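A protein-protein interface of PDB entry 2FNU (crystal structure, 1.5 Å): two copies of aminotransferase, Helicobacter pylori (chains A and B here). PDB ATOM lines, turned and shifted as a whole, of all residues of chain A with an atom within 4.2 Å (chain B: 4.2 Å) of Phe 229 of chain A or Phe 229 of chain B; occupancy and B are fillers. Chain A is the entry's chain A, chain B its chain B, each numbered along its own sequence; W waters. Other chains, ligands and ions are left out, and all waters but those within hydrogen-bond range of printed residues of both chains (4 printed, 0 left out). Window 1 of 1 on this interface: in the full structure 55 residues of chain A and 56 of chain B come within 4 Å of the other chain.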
ATOM      1  N   PHE A  53      -7.864   6.084  -3.524  1.00  0.00           N
ATOM      2  CA  PHE A  53      -7.596   7.045  -2.444  1.00  0.00           C
ATOM      3  C   PHE A  53      -8.389   8.315  -2.691  1.00  0.00           C
ATOM      4  O   PHE A  53      -8.875   8.543  -3.791  1.00  0.00           O
ATOM      5  CB  PHE A  53      -6.118   7.442  -2.465  1.00  0.00           C
ATOM      6  CG  PHE A  53      -5.185   6.328  -2.084  1.00  0.00           C
ATOM      7  CD1 PHE A  53      -4.674   6.263  -0.793  1.00  0.00           C
ATOM      8  CD2 PHE A  53      -4.829   5.345  -3.009  1.00  0.00           C
ATOM      9  CE1 PHE A  53      -3.822   5.242  -0.411  1.00  0.00           C
ATOM     10  CE2 PHE A  53      -3.957   4.314  -2.643  1.00  0.00           C
ATOM     11  CZ  PHE A  53      -3.470   4.261  -1.335  1.00  0.00           C
ATOM     12  N   ASN A  54      -8.452   9.193  -1.690  1.00  0.00           N
ATOM     13  CA  ASN A  54      -9.212  10.440  -1.841  1.00  0.00           C
ATOM     14  C   ASN A  54      -8.636  11.421  -2.867  1.00  0.00           C
ATOM     15  O   ASN A  54      -9.352  12.283  -3.362  1.00  0.00           O
ATOM     16  CB  ASN A  54      -9.357  11.148  -0.485  1.00  0.00           C
ATOM     17  CG  ASN A  54      -8.081  11.844  -0.041  1.00  0.00           C
ATOM     18  OD1 ASN A  54      -7.926  13.086  -0.203  1.00  0.00           O
ATOM     19  ND2 ASN A  54      -7.180  11.087   0.525  1.00  0.00           N
ATOM     20  N   SER A  58      -2.637  11.938  -1.911  1.00  0.00           N
ATOM     21  CA  SER A  58      -2.643  10.954  -0.817  1.00  0.00           C
ATOM     22  C   SER A  58      -2.042   9.630  -1.274  1.00  0.00           C
ATOM     23  O   SER A  58      -1.344   8.959  -0.513  1.00  0.00           O
ATOM     24  CB  SER A  58      -4.064  10.704  -0.336  1.00  0.00           C
ATOM     25  OG  SER A  58      -4.584  11.882   0.258  1.00  0.00           O
ATOM     26  N   LEU A  61       1.801  10.058  -1.316  1.00  0.00           N
ATOM     27  CA  LEU A  61       2.353   9.964   0.038  1.00  0.00           C
ATOM     28  C   LEU A  61       2.360   8.503   0.475  1.00  0.00           C
ATOM     29  O   LEU A  61       3.337   8.009   1.041  1.00  0.00           O
ATOM     30  CB  LEU A  61       1.506  10.763   1.031  1.00  0.00           C
ATOM     31  CG  LEU A  61       1.972  10.709   2.493  1.00  0.00           C
ATOM     32  CD1 LEU A  61       3.338  11.378   2.611  1.00  0.00           C
ATOM     33  CD2 LEU A  61       0.942  11.370   3.417  1.00  0.00           C
ATOM     34  N   THR A  62       1.247   7.807   0.252  1.00  0.00           N
ATOM     35  CA  THR A  62       1.151   6.402   0.671  1.00  0.00           C
ATOM     36  C   THR A  62       2.224   5.564  -0.021  1.00  0.00           C
ATOM     37  O   THR A  62       2.876   4.730   0.620  1.00  0.00           O
ATOM     38  CB  THR A  62      -0.245   5.870   0.409  1.00  0.00           C
ATOM     39  OG1 THR A  62      -1.183   6.628   1.185  1.00  0.00           O
ATOM     40  CG2 THR A  62      -0.369   4.400   0.823  1.00  0.00           C
ATOM     41  N   PHE A 207      -2.152   1.540   5.440  1.00  0.00           N
ATOM     42  CA  PHE A 207      -1.798   2.956   5.601  1.00  0.00           C
ATOM     43  C   PHE A 207      -2.951   3.882   5.222  1.00  0.00           C
ATOM     44  O   PHE A 207      -3.095   4.956   5.803  1.00  0.00           O
ATOM     45  CB  PHE A 207      -0.574   3.256   4.750  1.00  0.00           C
ATOM     46  CG  PHE A 207       0.075   4.588   5.011  1.00  0.00           C
ATOM     47  CD1 PHE A 207      -0.221   5.701   4.226  1.00  0.00           C
ATOM     48  CD2 PHE A 207       1.031   4.707   6.009  1.00  0.00           C
ATOM     49  CE1 PHE A 207       0.435   6.934   4.459  1.00  0.00           C
ATOM     50  CE2 PHE A 207       1.689   5.911   6.250  1.00  0.00           C
ATOM     51  CZ  PHE A 207       1.382   7.035   5.466  1.00  0.00           C
ATOM     52  N   ARG A 208      -3.763   3.449   4.261  1.00  0.00           N
ATOM     53  CA  ARG A 208      -4.916   4.224   3.789  1.00  0.00           C
ATOM     54  C   ARG A 208      -6.016   4.348   4.854  1.00  0.00           C
ATOM     55  O   ARG A 208      -6.838   5.279   4.801  1.00  0.00           O
ATOM     56  CB  ARG A 208      -5.481   3.539   2.538  1.00  0.00           C
ATOM     57  CG  ARG A 208      -6.686   4.231   1.929  1.00  0.00           C
ATOM     58  CD  ARG A 208      -7.232   3.487   0.723  1.00  0.00           C
ATOM     59  NE  ARG A 208      -7.705   2.138   1.073  1.00  0.00           N
ATOM     60  CZ  ARG A 208      -8.166   1.263   0.185  1.00  0.00           C
ATOM     61  NH1 ARG A 208      -8.247   1.576  -1.120  1.00  0.00           N
ATOM     62  NH2 ARG A 208      -8.553   0.049   0.586  1.00  0.00           N
ATOM     63  N   HIS A 227      -3.857   6.522   7.978  1.00  0.00           N
ATOM     64  CA  HIS A 227      -4.638   7.770   7.900  1.00  0.00           C
ATOM     65  C   HIS A 227      -6.070   7.417   7.505  1.00  0.00           C
ATOM     66  O   HIS A 227      -6.474   6.259   7.606  1.00  0.00           O
ATOM     67  CB  HIS A 227      -3.973   8.672   6.848  1.00  0.00           C
ATOM     68  CG  HIS A 227      -2.612   9.125   7.252  1.00  0.00           C
ATOM     69  ND1 HIS A 227      -2.373  10.388   7.747  1.00  0.00           N
ATOM     70  CD2 HIS A 227      -1.425   8.472   7.284  1.00  0.00           C
ATOM     71  CE1 HIS A 227      -1.090  10.504   8.048  1.00  0.00           C
ATOM     72  NE2 HIS A 227      -0.493   9.353   7.779  1.00  0.00           N
ATOM     73  N   ASN A 228      -6.834   8.397   7.037  1.00  0.00           N
ATOM     74  CA  ASN A 228      -8.076   8.101   6.347  1.00  0.00           C
ATOM     75  C   ASN A 228      -8.035   8.789   4.998  1.00  0.00           C
ATOM     76  O   ASN A 228      -8.463   9.944   4.852  1.00  0.00           O
ATOM     77  CB  ASN A 228      -9.332   8.497   7.168  1.00  0.00           C
ATOM     78  CG  ASN A 228     -10.655   8.211   6.439  1.00  0.00           C
ATOM     79  OD1 ASN A 228     -11.748   8.463   7.004  1.00  0.00           O
ATOM     80  ND2 ASN A 228     -10.582   7.730   5.200  1.00  0.00           N
ATOM     81  N   PHE A 229      -7.503   8.055   4.018  1.00  0.00           N
ATOM     82  CA  PHE A 229      -7.412   8.536   2.648  1.00  0.00           C
ATOM     83  C   PHE A 229      -8.364   7.731   1.767  1.00  0.00           C
ATOM     84  O   PHE A 229      -8.107   7.552   0.580  1.00  0.00           O
ATOM     85  CB  PHE A 229      -5.982   8.384   2.104  1.00  0.00           C
ATOM     86  CG  PHE A 229      -4.923   9.150   2.862  1.00  0.00           C
ATOM     87  CD1 PHE A 229      -5.194  10.355   3.487  1.00  0.00           C
ATOM     88  CD2 PHE A 229      -3.610   8.678   2.852  1.00  0.00           C
ATOM     89  CE1 PHE A 229      -4.174  11.065   4.157  1.00  0.00           C
ATOM     90  CE2 PHE A 229      -2.589   9.382   3.511  1.00  0.00           C
ATOM     91  CZ  PHE A 229      -2.877  10.583   4.150  1.00  0.00           C
ATOM     92  N   ARG A 230      -9.433   7.200   2.355  1.00  0.00           N
ATOM     93  CA  ARG A 230     -10.339   6.341   1.583  1.00  0.00           C
ATOM     94  C   ARG A 230     -11.101   7.137   0.520  1.00  0.00           C
ATOM     95  O   ARG A 230     -11.369   8.344   0.687  1.00  0.00           O
ATOM     96  CB  ARG A 230     -11.330   5.658   2.523  1.00  0.00           C
ATOM     97  CG  ARG A 230     -10.655   4.729   3.533  1.00  0.00           C
ATOM     98  CD  ARG A 230     -11.701   3.918   4.280  1.00  0.00           C
ATOM     99  NE  ARG A 230     -12.620   4.745   5.061  1.00  0.00           N
ATOM    100  CZ  ARG A 230     -12.590   4.892   6.390  1.00  0.00           C
ATOM    101  NH1 ARG A 230     -11.658   4.280   7.146  1.00  0.00           N
ATOM    102  NH2 ARG A 230     -13.498   5.662   6.973  1.00  0.00           N
ATOM    103  N   LEU A 231     -11.473   6.436  -0.556  1.00  0.00           N
ATOM    104  CA  LEU A 231     -12.432   6.943  -1.537  1.00  0.00           C
ATOM    105  C   LEU A 231     -13.799   6.367  -1.183  1.00  0.00           C
ATOM    106  O   LEU A 231     -13.938   5.163  -0.981  1.00  0.00           O
ATOM    107  CB  LEU A 231     -12.044   6.514  -2.968  1.00  0.00           C
ATOM    108  CG  LEU A 231     -12.746   7.210  -4.129  1.00  0.00           C
ATOM    109  CD1 LEU A 231     -12.290   8.650  -4.216  1.00  0.00           C
ATOM    110  CD2 LEU A 231     -12.503   6.477  -5.450  1.00  0.00           C
ATOM    111  N   PHE B  53     -12.518  19.042   5.028  1.00  0.00           N
ATOM    112  CA  PHE B  53     -11.433  18.125   4.623  1.00  0.00           C
ATOM    113  C   PHE B  53     -12.041  16.814   4.162  1.00  0.00           C
ATOM    114  O   PHE B  53     -13.229  16.558   4.437  1.00  0.00           O
ATOM    115  CB  PHE B  53     -10.538  17.804   5.829  1.00  0.00           C
ATOM    116  CG  PHE B  53      -9.684  18.949   6.284  1.00  0.00           C
ATOM    117  CD1 PHE B  53      -8.363  19.054   5.883  1.00  0.00           C
ATOM    118  CD2 PHE B  53     -10.215  19.935   7.114  1.00  0.00           C
ATOM    119  CE1 PHE B  53      -7.576  20.126   6.300  1.00  0.00           C
ATOM    120  CE2 PHE B  53      -9.441  21.004   7.530  1.00  0.00           C
ATOM    121  CZ  PHE B  53      -8.119  21.105   7.128  1.00  0.00           C
ATOM    122  N   ASN B  54     -11.234  15.958   3.516  1.00  0.00           N
ATOM    123  CA  ASN B  54     -11.761  14.690   3.019  1.00  0.00           C
ATOM    124  C   ASN B  54     -12.176  13.723   4.136  1.00  0.00           C
ATOM    125  O   ASN B  54     -12.934  12.793   3.908  1.00  0.00           O
ATOM    126  CB  ASN B  54     -10.749  13.998   2.091  1.00  0.00           C
ATOM    127  CG  ASN B  54      -9.591  13.402   2.843  1.00  0.00           C
ATOM    128  OD1 ASN B  54      -9.563  12.168   3.119  1.00  0.00           O
ATOM    129  ND2 ASN B  54      -8.662  14.240   3.227  1.00  0.00           N
ATOM    130  N   SER B  58      -7.758  13.524   8.339  1.00  0.00           N
ATOM    131  CA  SER B  58      -6.993  14.556   7.624  1.00  0.00           C
ATOM    132  C   SER B  58      -7.026  15.891   8.359  1.00  0.00           C
ATOM    133  O   SER B  58      -6.003  16.601   8.440  1.00  0.00           O
ATOM    134  CB  SER B  58      -7.488  14.727   6.187  1.00  0.00           C
ATOM    135  OG  SER B  58      -7.230  13.561   5.426  1.00  0.00           O
ATOM    136  N   LEU B  61      -4.684  15.636  11.412  1.00  0.00           N
ATOM    137  CA  LEU B  61      -3.275  15.772  11.047  1.00  0.00           C
ATOM    138  C   LEU B  61      -2.970  17.240  10.749  1.00  0.00           C
ATOM    139  O   LEU B  61      -1.951  17.785  11.182  1.00  0.00           O
ATOM    140  CB  LEU B  61      -2.944  14.956   9.801  1.00  0.00           C
ATOM    141  CG  LEU B  61      -1.513  15.139   9.273  1.00  0.00           C
ATOM    142  CD1 LEU B  61      -0.513  14.537  10.270  1.00  0.00           C
ATOM    143  CD2 LEU B  61      -1.348  14.495   7.897  1.00  0.00           C
ATOM    144  N   THR B  62      -3.853  17.880   9.994  1.00  0.00           N
ATOM    145  CA  THR B  62      -3.638  19.286   9.628  1.00  0.00           C
ATOM    146  C   THR B  62      -3.581  20.185  10.866  1.00  0.00           C
ATOM    147  O   THR B  62      -2.725  21.067  10.963  1.00  0.00           O
ATOM    148  CB  THR B  62      -4.745  19.746   8.670  1.00  0.00           C
ATOM    149  OG1 THR B  62      -4.677  18.924   7.498  1.00  0.00           O
ATOM    150  CG2 THR B  62      -4.558  21.219   8.261  1.00  0.00           C
ATOM    151  N   PHE B 207      -2.146  24.099   3.983  1.00  0.00           N
ATOM    152  CA  PHE B 207      -1.695  22.705   4.199  1.00  0.00           C
ATOM    153  C   PHE B 207      -2.645  21.716   3.542  1.00  0.00           C
ATOM    154  O   PHE B 207      -2.222  20.635   3.095  1.00  0.00           O
ATOM    155  CB  PHE B 207      -1.611  22.442   5.694  1.00  0.00           C
ATOM    156  CG  PHE B 207      -0.933  21.146   6.076  1.00  0.00           C
ATOM    157  CD1 PHE B 207      -1.691  19.991   6.330  1.00  0.00           C
ATOM    158  CD2 PHE B 207       0.457  21.097   6.257  1.00  0.00           C
ATOM    159  CE1 PHE B 207      -1.071  18.808   6.748  1.00  0.00           C
ATOM    160  CE2 PHE B 207       1.083  19.930   6.658  1.00  0.00           C
ATOM    161  CZ  PHE B 207       0.318  18.782   6.900  1.00  0.00           C
ATOM    162  N   ARG B 208      -3.927  22.084   3.491  1.00  0.00           N
ATOM    163  CA  ARG B 208      -4.968  21.255   2.877  1.00  0.00           C
ATOM    164  C   ARG B 208      -4.807  21.101   1.356  1.00  0.00           C
ATOM    165  O   ARG B 208      -5.314  20.148   0.765  1.00  0.00           O
ATOM    166  CB  ARG B 208      -6.339  21.858   3.205  1.00  0.00           C
ATOM    167  CG  ARG B 208      -7.533  21.096   2.612  1.00  0.00           C
ATOM    168  CD  ARG B 208      -8.875  21.764   2.948  1.00  0.00           C
ATOM    169  NE  ARG B 208      -8.951  23.096   2.333  1.00  0.00           N
ATOM    170  CZ  ARG B 208      -9.971  23.936   2.480  1.00  0.00           C
ATOM    171  NH1 ARG B 208     -11.046  23.593   3.203  1.00  0.00           N
ATOM    172  NH2 ARG B 208      -9.925  25.120   1.874  1.00  0.00           N
ATOM    173  N   HIS B 227      -0.894  19.142   1.173  1.00  0.00           N
ATOM    174  CA  HIS B 227      -1.383  17.862   0.670  1.00  0.00           C
ATOM    175  C   HIS B 227      -2.598  18.125  -0.212  1.00  0.00           C
ATOM    176  O   HIS B 227      -2.801  19.245  -0.674  1.00  0.00           O
ATOM    177  CB  HIS B 227      -1.754  16.972   1.867  1.00  0.00           C
ATOM    178  CG  HIS B 227      -0.577  16.592   2.714  1.00  0.00           C
ATOM    179  ND1 HIS B 227      -0.030  15.332   2.682  1.00  0.00           N
ATOM    180  CD2 HIS B 227       0.154  17.297   3.623  1.00  0.00           C
ATOM    181  CE1 HIS B 227       1.000  15.272   3.509  1.00  0.00           C
ATOM    182  NE2 HIS B 227       1.136  16.449   4.092  1.00  0.00           N
ATOM    183  N   ASN B 228      -3.382  17.094  -0.508  1.00  0.00           N
ATOM    184  CA  ASN B 228      -4.701  17.328  -1.113  1.00  0.00           C
ATOM    185  C   ASN B 228      -5.701  16.575  -0.257  1.00  0.00           C
ATOM    186  O   ASN B 228      -5.963  15.379  -0.485  1.00  0.00           O
ATOM    187  CB  ASN B 228      -4.776  16.846  -2.576  1.00  0.00           C
ATOM    188  CG  ASN B 228      -6.162  17.029  -3.196  1.00  0.00           C
ATOM    189  OD1 ASN B 228      -6.357  16.770  -4.404  1.00  0.00           O
ATOM    190  ND2 ASN B 228      -7.120  17.448  -2.402  1.00  0.00           N
ATOM    191  N   PHE B 229      -6.179  17.284   0.771  1.00  0.00           N
ATOM    192  CA  PHE B 229      -7.205  16.784   1.686  1.00  0.00           C
ATOM    193  C   PHE B 229      -8.526  17.522   1.444  1.00  0.00           C
ATOM    194  O   PHE B 229      -9.336  17.682   2.352  1.00  0.00           O
ATOM    195  CB  PHE B 229      -6.769  17.002   3.141  1.00  0.00           C
ATOM    196  CG  PHE B 229      -5.490  16.295   3.529  1.00  0.00           C
ATOM    197  CD1 PHE B 229      -5.116  15.081   2.949  1.00  0.00           C
ATOM    198  CD2 PHE B 229      -4.718  16.812   4.566  1.00  0.00           C
ATOM    199  CE1 PHE B 229      -3.941  14.428   3.354  1.00  0.00           C
ATOM    200  CE2 PHE B 229      -3.545  16.167   4.973  1.00  0.00           C
ATOM    201  CZ  PHE B 229      -3.166  14.975   4.386  1.00  0.00           C
ATOM    202  N   ARG B 230      -8.746  17.983   0.217  1.00  0.00           N
ATOM    203  CA  ARG B 230      -9.934  18.795  -0.059  1.00  0.00           C
ATOM    204  C   ARG B 230     -11.201  17.958  -0.011  1.00  0.00           C
ATOM    205  O   ARG B 230     -11.192  16.747  -0.315  1.00  0.00           O
ATOM    206  CB  ARG B 230      -9.801  19.462  -1.426  1.00  0.00           C
ATOM    207  CG  ARG B 230      -8.619  20.437  -1.513  1.00  0.00           C
ATOM    208  CD  ARG B 230      -8.639  21.229  -2.806  1.00  0.00           C
ATOM    209  NE  ARG B 230      -8.548  20.365  -3.995  1.00  0.00           N
ATOM    210  CZ  ARG B 230      -7.495  20.275  -4.809  1.00  0.00           C
ATOM    211  NH1 ARG B 230      -6.385  20.994  -4.609  1.00  0.00           N
ATOM    212  NH2 ARG B 230      -7.566  19.480  -5.874  1.00  0.00           N
ATOM    213  N   LEU B 231     -12.297  18.613   0.383  1.00  0.00           N
ATOM    214  CA  LEU B 231     -13.628  18.052   0.237  1.00  0.00           C
ATOM    215  C   LEU B 231     -14.194  18.562  -1.088  1.00  0.00           C
ATOM    216  O   LEU B 231     -14.177  19.767  -1.350  1.00  0.00           O
ATOM    217  CB  LEU B 231     -14.513  18.519   1.394  1.00  0.00           C
ATOM    218  CG  LEU B 231     -15.848  17.761   1.535  1.00  0.00           C
ATOM    219  CD1 LEU B 231     -15.590  16.333   2.042  1.00  0.00           C
ATOM    220  CD2 LEU B 231     -16.793  18.477   2.497  1.00  0.00           C
HETATM  221  O   HOH W   1      -9.226  15.288  -1.605  1.00  0.00           O
HETATM  222  O   HOH W   2      -6.416  11.170   6.774  1.00  0.00           O
HETATM  223  O   HOH W   3      -3.107  14.312   0.008  1.00  0.00           O
HETATM  224  O   HOH W   4     -11.400   9.873   3.046  1.00  0.00           O
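The backbone carbonyl oxygen (O) of Ser 58 of chain A lies within hydrogen-bond range of the side-chain hydroxyl (OG1) of Thr 62 of chain A, 2.9 Å away.
O of Ser 58 of chain B is in hydrogen-bond range of OG1 of Thr 62 of chain B (2.8 Å).
The backbone NH (N) of Asn 54 of chain A lies within hydrogen-bond range of the backbone carbonyl oxygen (O) of Phe 229 of chain A (2.8 Å).
The backbone NH (N) of Arg 230 of chain B sits close to the side-chain amide nitrogen (ND2) of Asn 228 of chain B (3.1 Å).
The backbone NH (N) of His 227 of chain B lies within hydrogen-bond range of the backbone carbonyl oxygen (O) of Phe 207 of chain B.
The backbone carbonyl oxygen of Arg 208 of chain A is in hydrogen-bond range of the backbone NH of Phe 229 of chain A.
Water W1 lies within hydrogen-bond range of the backbone carbonyl oxygen of Arg 230 of chain B, the side-chain amide oxygen of Asn 54 of chain A and the side-chain amide nitrogen of Asn 228 of chain B.
Water W4 lies within hydrogen-bond range of O of Arg 230 of chain A, OD1 of Asn 54 of chain B and ND2 of Asn 228 of chain A.
Water W2 lies within hydrogen-bond range of N of Asn 228 of chain A (2.8 Å) and OG of Ser 58 of chain B (2.9 Å).
Water W3 lies within hydrogen-bond range of the backbone NH of Asn 228 of chain B (2.8 Å) and the side-chain hydroxyl of Ser 58 of chain A (2.9 Å).
Asn 54 of chain B touches its own counterpart, Asn 54 of chain A.
Asn 54 of chain A touches Asn 228 of chain B, and with the chains exchanged Asn 228 of chain A touches Asn 54 of chain B.
Ser 58 of chain A touches Asn 228 of chain B, and with the chains exchanged Asn 228 of chain A touches Ser 58 of chain B.
Leu 61 of chain A touches His 227 of chain B, but with the chains exchanged His 227 of chain A does not touch Leu 61 of chain B (4.002 Å).
12 positions are printed for both chains.
Asn 54 of chain B touches Asn 54 of chain A (CG to OD1, 3.5 Å).
OG of Ser 58 of chain A touches O of Asn 228 of chain B, at 3.8 Å.
Leu 61 of chain A touches His 227 of chain B.
O of Asn 228 of chain A touches OG of Ser 58 of chain B (3.9 Å).
Phe 229 of chain B touches Phe 229 of chain A.
Of the 12 printed residues of chain A, 5 touch a printed residue of chain B.
Hydrophobic or aromatic side chains of chain A that line the printed part of chain B: Leu 61 and Phe 229.
Of the 12 printed residues of chain B, 5 touch a printed residue of chain A.
Among the printed residues, 7 pairs touch across the chains.
Among the printed residues, no Asp or Glu carboxylate lies within 4 Å of a Lys or Arg side-chain nitrogen of the other chain.
The side-chain amide oxygen (OD1) of Asn 54 of chain A sits close to the backbone carbonyl oxygen (O) of Asn 228 of chain B (3.0 Å).
O of Asn 228 of chain A sits close to OD1 of Asn 54 of chain B, 3.0 Å away.
Printed residues of chain A within 4 Å of Ser 58 of chain B: Asn 228 (3.9 Å).
Printed residues of chain A within 4 Å of Asn 54 of chain B: Asn 54 (3.5 Å) and Asn 228 (3.0 Å).
Printed residues of chain B within 4 Å of Ser 58 of chain A: Asn 228 (3.8 Å).
Arg 208 of chain B touches none of the printed residues of chain A.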
